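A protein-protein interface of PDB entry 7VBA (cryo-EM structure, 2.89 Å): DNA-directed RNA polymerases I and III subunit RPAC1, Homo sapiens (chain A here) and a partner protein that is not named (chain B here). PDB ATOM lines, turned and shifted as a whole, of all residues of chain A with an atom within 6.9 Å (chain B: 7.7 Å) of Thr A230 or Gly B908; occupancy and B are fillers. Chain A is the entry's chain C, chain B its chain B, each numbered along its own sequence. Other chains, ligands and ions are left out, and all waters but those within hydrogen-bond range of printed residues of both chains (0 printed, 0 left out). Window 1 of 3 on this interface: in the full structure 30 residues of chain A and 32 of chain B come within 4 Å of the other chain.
N of Tyr B980 lies within hydrogen-bond range of O of Phe B904, at 2.7 Å.
The backbone NH of Glu A311 lies within hydrogen-bond range of the backbone carbonyl oxygen of Thr A230, at 3.3 Å.
The backbone NH (N) of Ser A309 is in hydrogen-bond range of the backbone carbonyl oxygen (O) of Ser A232, 3.3 Å away.
Gly B908 touches just these residues of chain A: Thr A230 and Ser A232.
No residue of chain B comes within 4 Å of Ala A229.
Of the printed residues of chain B, Tyr A233 touches Phe B904 (3.6 Å).
Of the printed residues of chain B, Arg A77 touches Phe B904 (3.6 Å).
Printed residues of chain B within 4 Å of Ser A232: Phe B904 and Gly B908.
Glu B977 touches none of the printed residues of chain A.
Ser A312 touches none of the printed residues of chain B.
The nearest residue of chain B that does not touch Thr A230 is Met B909 (5.4 Å).
The nearest residue of chain A that does not touch Gly B908 is Ala A231 (6.0 Å).
NE of Arg A77 touches CE1 of Phe B904, at 3.6 Å.
O of Gly B908 touches CG2 of Thr A230, 3.6 Å away.
Ser A232 touches Phe B904 (CB to CD2, 3.9 Å).
Ser A232 touches Gly B908.
CE2 of Phe B904 touches O of Tyr A233, 3.6 Å away.
Of the 12 printed residues of chain B, 2 touch a printed residue of chain A.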
ATOM      1  N   ARG A  77      -6.033  27.901   0.813  1.00  0.00           N
ATOM      2  CA  ARG A  77      -5.364  26.911   1.654  1.00  0.00           C
ATOM      3  C   ARG A  77      -5.929  26.909   3.070  1.00  0.00           C
ATOM      4  O   ARG A  77      -6.175  25.844   3.647  1.00  0.00           O
ATOM      5  CB  ARG A  77      -3.861  27.181   1.671  1.00  0.00           C
ATOM      6  CG  ARG A  77      -3.054  26.197   2.479  1.00  0.00           C
ATOM      7  CD  ARG A  77      -1.717  26.787   2.866  1.00  0.00           C
ATOM      8  NE  ARG A  77      -1.858  27.859   3.843  1.00  0.00           N
ATOM      9  CZ  ARG A  77      -1.722  27.699   5.153  1.00  0.00           C
ATOM     10  NH1 ARG A  77      -1.442  26.506   5.650  1.00  0.00           N
ATOM     11  NH2 ARG A  77      -1.867  28.732   5.966  1.00  0.00           N
ATOM     12  N   LEU A  80      -9.484  25.153   3.290  1.00  0.00           N
ATOM     13  CA  LEU A  80      -9.508  23.685   3.282  1.00  0.00           C
ATOM     14  C   LEU A  80      -9.111  23.162   4.660  1.00  0.00           C
ATOM     15  O   LEU A  80      -9.839  22.325   5.190  1.00  0.00           O
ATOM     16  CB  LEU A  80      -8.598  23.219   2.150  1.00  0.00           C
ATOM     17  CG  LEU A  80      -9.215  23.259   0.761  1.00  0.00           C
ATOM     18  CD1 LEU A  80      -8.155  23.481  -0.295  1.00  0.00           C
ATOM     19  CD2 LEU A  80      -9.970  21.978   0.494  1.00  0.00           C
ATOM     20  N   LEU A  81      -8.058  23.686   5.263  1.00  0.00           N
ATOM     21  CA  LEU A  81      -7.596  23.233   6.594  1.00  0.00           C
ATOM     22  C   LEU A  81      -8.619  23.538   7.676  1.00  0.00           C
ATOM     23  O   LEU A  81      -8.888  22.649   8.444  1.00  0.00           O
ATOM     24  CB  LEU A  81      -6.256  23.885   6.938  1.00  0.00           C
ATOM     25  CG  LEU A  81      -5.042  23.457   6.126  1.00  0.00           C
ATOM     26  CD1 LEU A  81      -3.835  24.258   6.563  1.00  0.00           C
ATOM     27  CD2 LEU A  81      -4.774  21.977   6.308  1.00  0.00           C
ATOM     28  N   VAL A 228      -8.876  17.409   5.451  1.00  0.00           N
ATOM     29  CA  VAL A 228      -7.677  17.197   4.601  1.00  0.00           C
ATOM     30  C   VAL A 228      -6.470  16.867   5.464  1.00  0.00           C
ATOM     31  O   VAL A 228      -6.408  17.414   6.548  1.00  0.00           O
ATOM     32  CB  VAL A 228      -7.387  18.472   3.785  1.00  0.00           C
ATOM     33  CG1 VAL A 228      -8.410  18.746   2.704  1.00  0.00           C
ATOM     34  CG2 VAL A 228      -7.180  19.698   4.648  1.00  0.00           C
ATOM     35  N   ALA A 229      -5.610  15.933   5.052  1.00  0.00           N
ATOM     36  CA  ALA A 229      -4.332  15.742   5.727  1.00  0.00           C
ATOM     37  C   ALA A 229      -3.514  17.024   5.675  1.00  0.00           C
ATOM     38  O   ALA A 229      -3.221  17.636   6.707  1.00  0.00           O
ATOM     39  CB  ALA A 229      -3.565  14.585   5.092  1.00  0.00           C
ATOM     40  N   THR A 230      -3.151  17.457   4.470  1.00  0.00           N
ATOM     41  CA  THR A 230      -2.575  18.775   4.267  1.00  0.00           C
ATOM     42  C   THR A 230      -3.088  19.336   2.952  1.00  0.00           C
ATOM     43  O   THR A 230      -3.417  18.590   2.028  1.00  0.00           O
ATOM     44  CB  THR A 230      -1.044  18.747   4.261  1.00  0.00           C
ATOM     45  OG1 THR A 230      -0.588  17.740   3.351  1.00  0.00           O
ATOM     46  CG2 THR A 230      -0.515  18.456   5.651  1.00  0.00           C
ATOM     47  N   ALA A 231      -3.152  20.664   2.879  1.00  0.00           N
ATOM     48  CA  ALA A 231      -3.639  21.363   1.699  1.00  0.00           C
ATOM     49  C   ALA A 231      -2.675  22.461   1.278  1.00  0.00           C
ATOM     50  O   ALA A 231      -3.079  23.445   0.657  1.00  0.00           O
ATOM     51  CB  ALA A 231      -5.032  21.940   1.946  1.00  0.00           C
ATOM     52  N   SER A 232      -1.396  22.303   1.601  1.00  0.00           N
ATOM     53  CA  SER A 232      -0.428  23.358   1.367  1.00  0.00           C
ATOM     54  C   SER A 232      -0.237  23.606  -0.127  1.00  0.00           C
ATOM     55  O   SER A 232      -0.778  22.904  -0.983  1.00  0.00           O
ATOM     56  CB  SER A 232       0.907  23.007   2.013  1.00  0.00           C
ATOM     57  OG  SER A 232       1.412  21.794   1.486  1.00  0.00           O
ATOM     58  N   TYR A 233       0.563  24.615  -0.458  1.00  0.00           N
ATOM     59  CA  TYR A 233       0.935  24.983  -1.837  1.00  0.00           C
ATOM     60  C   TYR A 233       2.386  25.430  -1.836  1.00  0.00           C
ATOM     61  O   TYR A 233       2.916  25.654  -0.779  1.00  0.00           O
ATOM     62  CB  TYR A 233       0.169  26.210  -2.298  1.00  0.00           C
ATOM     63  CG  TYR A 233       0.267  27.493  -1.521  1.00  0.00           C
ATOM     64  CD1 TYR A 233       1.407  28.270  -1.552  1.00  0.00           C
ATOM     65  CD2 TYR A 233      -0.834  27.979  -0.848  1.00  0.00           C
ATOM     66  CE1 TYR A 233       1.485  29.460  -0.859  1.00  0.00           C
ATOM     67  CE2 TYR A 233      -0.776  29.169  -0.153  1.00  0.00           C
ATOM     68  CZ  TYR A 233       0.385  29.908  -0.163  1.00  0.00           C
ATOM     69  OH  TYR A 233       0.444  31.081   0.512  1.00  0.00           O
ATOM     70  N   SER A 309      -1.627  20.930  -3.440  1.00  0.00           N
ATOM     71  CA  SER A 309      -1.670  19.496  -3.174  1.00  0.00           C
ATOM     72  C   SER A 309      -2.655  19.270  -2.040  1.00  0.00           C
ATOM     73  O   SER A 309      -2.350  19.582  -0.888  1.00  0.00           O
ATOM     74  CB  SER A 309      -0.294  18.959  -2.811  1.00  0.00           C
ATOM     75  OG  SER A 309      -0.069  19.083  -1.420  1.00  0.00           O
ATOM     76  N   VAL A 310      -3.824  18.731  -2.362  1.00  0.00           N
ATOM     77  CA  VAL A 310      -4.871  18.469  -1.384  1.00  0.00           C
ATOM     78  C   VAL A 310      -5.009  16.963  -1.225  1.00  0.00           C
ATOM     79  O   VAL A 310      -5.125  16.237  -2.219  1.00  0.00           O
ATOM     80  CB  VAL A 310      -6.204  19.106  -1.807  1.00  0.00           C
ATOM     81  CG1 VAL A 310      -7.282  18.803  -0.789  1.00  0.00           C
ATOM     82  CG2 VAL A 310      -6.036  20.598  -1.988  1.00  0.00           C
ATOM     83  N   GLU A 311      -4.991  16.495   0.020  1.00  0.00           N
ATOM     84  CA  GLU A 311      -5.132  15.077   0.335  1.00  0.00           C
ATOM     85  C   GLU A 311      -6.218  14.934   1.389  1.00  0.00           C
ATOM     86  O   GLU A 311      -6.015  15.314   2.544  1.00  0.00           O
ATOM     87  CB  GLU A 311      -3.816  14.485   0.833  1.00  0.00           C
ATOM     88  CG  GLU A 311      -2.611  14.881   0.009  1.00  0.00           C
ATOM     89  CD  GLU A 311      -1.324  14.823   0.803  1.00  0.00           C
ATOM     90  OE1 GLU A 311      -1.154  13.872   1.595  1.00  0.00           O
ATOM     91  OE2 GLU A 311      -0.483  15.731   0.639  1.00  0.00           O
ATOM     92  N   SER A 312      -7.363  14.390   0.997  1.00  0.00           N
ATOM     93  CA  SER A 312      -8.463  14.255   1.933  1.00  0.00           C
ATOM     94  C   SER A 312      -8.292  13.006   2.787  1.00  0.00           C
ATOM     95  O   SER A 312      -7.590  12.061   2.424  1.00  0.00           O
ATOM     96  CB  SER A 312      -9.800  14.205   1.199  1.00  0.00           C
ATOM     97  OG  SER A 312      -9.860  13.082   0.341  1.00  0.00           O
ATOM     98  N   ARG B 766      -4.902  16.583  18.497  1.00  0.00           N
ATOM     99  CA  ARG B 766      -4.713  15.226  18.010  1.00  0.00           C
ATOM    100  C   ARG B 766      -4.000  14.337  19.016  1.00  0.00           C
ATOM    101  O   ARG B 766      -3.532  13.257  18.648  1.00  0.00           O
ATOM    102  CB  ARG B 766      -3.938  15.235  16.697  1.00  0.00           C
ATOM    103  CG  ARG B 766      -4.752  15.627  15.491  1.00  0.00           C
ATOM    104  CD  ARG B 766      -3.838  16.045  14.371  1.00  0.00           C
ATOM    105  NE  ARG B 766      -4.543  16.754  13.316  1.00  0.00           N
ATOM    106  CZ  ARG B 766      -4.036  17.783  12.653  1.00  0.00           C
ATOM    107  NH1 ARG B 766      -2.826  18.229  12.944  1.00  0.00           N
ATOM    108  NH2 ARG B 766      -4.746  18.374  11.705  1.00  0.00           N
ATOM    109  N   PRO B 903       3.603  28.576  10.187  1.00  0.00           N
ATOM    110  CA  PRO B 903       4.372  28.649   8.938  1.00  0.00           C
ATOM    111  C   PRO B 903       4.584  27.259   8.358  1.00  0.00           C
ATOM    112  O   PRO B 903       5.288  26.433   8.940  1.00  0.00           O
ATOM    113  CB  PRO B 903       5.691  29.290   9.377  1.00  0.00           C
ATOM    114  CG  PRO B 903       5.828  28.913  10.798  1.00  0.00           C
ATOM    115  CD  PRO B 903       4.443  28.819  11.370  1.00  0.00           C
ATOM    116  N   PHE B 904       3.976  27.001   7.207  1.00  0.00           N
ATOM    117  CA  PHE B 904       4.102  25.704   6.568  1.00  0.00           C
ATOM    118  C   PHE B 904       5.349  25.663   5.701  1.00  0.00           C
ATOM    119  O   PHE B 904       5.758  26.667   5.118  1.00  0.00           O
ATOM    120  CB  PHE B 904       2.872  25.376   5.723  1.00  0.00           C
ATOM    121  CG  PHE B 904       2.518  26.431   4.717  1.00  0.00           C
ATOM    122  CD1 PHE B 904       1.945  27.621   5.112  1.00  0.00           C
ATOM    123  CD2 PHE B 904       2.740  26.221   3.373  1.00  0.00           C
ATOM    124  CE1 PHE B 904       1.612  28.580   4.188  1.00  0.00           C
ATOM    125  CE2 PHE B 904       2.408  27.178   2.450  1.00  0.00           C
ATOM    126  CZ  PHE B 904       1.847  28.358   2.860  1.00  0.00           C
ATOM    127  N   THR B 905       5.950  24.487   5.620  1.00  0.00           N
ATOM    128  CA  THR B 905       7.173  24.291   4.865  1.00  0.00           C
ATOM    129  C   THR B 905       6.843  23.954   3.416  1.00  0.00           C
ATOM    130  O   THR B 905       5.693  23.707   3.048  1.00  0.00           O
ATOM    131  CB  THR B 905       8.027  23.203   5.517  1.00  0.00           C
ATOM    132  OG1 THR B 905       9.268  23.081   4.814  1.00  0.00           O
ATOM    133  CG2 THR B 905       7.306  21.880   5.494  1.00  0.00           C
ATOM    134  N   GLU B 906       7.878  23.944   2.576  1.00  0.00           N
ATOM    135  CA  GLU B 906       7.670  23.666   1.160  1.00  0.00           C
ATOM    136  C   GLU B 906       7.328  22.204   0.917  1.00  0.00           C
ATOM    137  O   GLU B 906       7.025  21.820  -0.216  1.00  0.00           O
ATOM    138  CB  GLU B 906       8.911  24.059   0.363  1.00  0.00           C
ATOM    139  CG  GLU B 906       8.657  24.217  -1.118  1.00  0.00           C
ATOM    140  CD  GLU B 906       9.931  24.432  -1.902  1.00  0.00           C
ATOM    141  OE1 GLU B 906      11.021  24.314  -1.304  1.00  0.00           O
ATOM    142  OE2 GLU B 906       9.844  24.724  -3.114  1.00  0.00           O
ATOM    143  N   SER B 907       7.380  21.377   1.957  1.00  0.00           N
ATOM    144  CA  SER B 907       7.012  19.972   1.861  1.00  0.00           C
ATOM    145  C   SER B 907       5.597  19.701   2.349  1.00  0.00           C
ATOM    146  O   SER B 907       5.187  18.538   2.395  1.00  0.00           O
ATOM    147  CB  SER B 907       7.998  19.120   2.657  1.00  0.00           C
ATOM    148  OG  SER B 907       9.312  19.255   2.150  1.00  0.00           O
ATOM    149  N   GLY B 908       4.845  20.737   2.706  1.00  0.00           N
ATOM    150  CA  GLY B 908       3.512  20.580   3.238  1.00  0.00           C
ATOM    151  C   GLY B 908       3.446  20.487   4.744  1.00  0.00           C
ATOM    152  O   GLY B 908       2.364  20.674   5.314  1.00  0.00           O
ATOM    153  N   MET B 909       4.565  20.207   5.403  1.00  0.00           N
ATOM    154  CA  MET B 909       4.565  20.013   6.841  1.00  0.00           C
ATOM    155  C   MET B 909       4.230  21.315   7.558  1.00  0.00           C
ATOM    156  O   MET B 909       4.128  22.385   6.959  1.00  0.00           O
ATOM    157  CB  MET B 909       5.923  19.496   7.310  1.00  0.00           C
ATOM    158  CG  MET B 909       6.256  18.089   6.860  1.00  0.00           C
ATOM    159  SD  MET B 909       7.636  17.443   7.802  1.00  0.00           S
ATOM    160  CE  MET B 909       7.198  18.050   9.424  1.00  0.00           C
ATOM    161  N   VAL B 910       4.074  21.212   8.872  1.00  0.00           N
ATOM    162  CA  VAL B 910       3.788  22.359   9.724  1.00  0.00           C
ATOM    163  C   VAL B 910       4.294  22.025  11.120  1.00  0.00           C
ATOM    164  O   VAL B 910       3.839  21.042  11.717  1.00  0.00           O
ATOM    165  CB  VAL B 910       2.288  22.691   9.739  1.00  0.00           C
ATOM    166  CG1 VAL B 910       1.970  23.630  10.877  1.00  0.00           C
ATOM    167  CG2 VAL B 910       1.870  23.306   8.425  1.00  0.00           C
ATOM    168  N   PRO B 911       5.222  22.797  11.679  1.00  0.00           N
ATOM    169  CA  PRO B 911       5.745  22.464  13.005  1.00  0.00           C
ATOM    170  C   PRO B 911       4.624  22.332  14.020  1.00  0.00           C
ATOM    171  O   PRO B 911       3.517  22.840  13.840  1.00  0.00           O
ATOM    172  CB  PRO B 911       6.658  23.650  13.334  1.00  0.00           C
ATOM    173  CG  PRO B 911       6.207  24.740  12.428  1.00  0.00           C
ATOM    174  CD  PRO B 911       5.788  24.055  11.173  1.00  0.00           C
ATOM    175  N   GLU B 977      15.180  24.271   6.167  1.00  0.00           N
ATOM    176  CA  GLU B 977      14.191  24.222   5.106  1.00  0.00           C
ATOM    177  C   GLU B 977      13.407  25.523   5.133  1.00  0.00           C
ATOM    178  O   GLU B 977      13.162  26.088   6.201  1.00  0.00           O
ATOM    179  CB  GLU B 977      13.247  23.027   5.279  1.00  0.00           C
ATOM    180  CG  GLU B 977      12.152  22.918   4.226  1.00  0.00           C
ATOM    181  CD  GLU B 977      12.681  22.569   2.843  1.00  0.00           C
ATOM    182  OE1 GLU B 977      13.742  21.915   2.752  1.00  0.00           O
ATOM    183  OE2 GLU B 977      12.034  22.948   1.845  1.00  0.00           O
ATOM    184  N   TYR B 980       6.821  29.026   4.478  1.00  0.00           N
ATOM    185  CA  TYR B 980       5.938  30.109   4.086  1.00  0.00           C
ATOM    186  C   TYR B 980       5.257  30.664   5.326  1.00  0.00           C
ATOM    187  O   TYR B 980       5.209  30.016   6.372  1.00  0.00           O
ATOM    188  CB  TYR B 980       4.881  29.642   3.080  1.00  0.00           C
ATOM    189  CG  TYR B 980       5.432  29.255   1.734  1.00  0.00           C
ATOM    190  CD1 TYR B 980       6.209  28.121   1.584  1.00  0.00           C
ATOM    191  CD2 TYR B 980       5.170  30.022   0.612  1.00  0.00           C
ATOM    192  CE1 TYR B 980       6.715  27.764   0.361  1.00  0.00           C
ATOM    193  CE2 TYR B 980       5.672  29.675  -0.615  1.00  0.00           C
ATOM    194  CZ  TYR B 980       6.445  28.544  -0.735  1.00  0.00           C
ATOM    195  OH  TYR B 980       6.951  28.187  -1.959  1.00  0.00           O
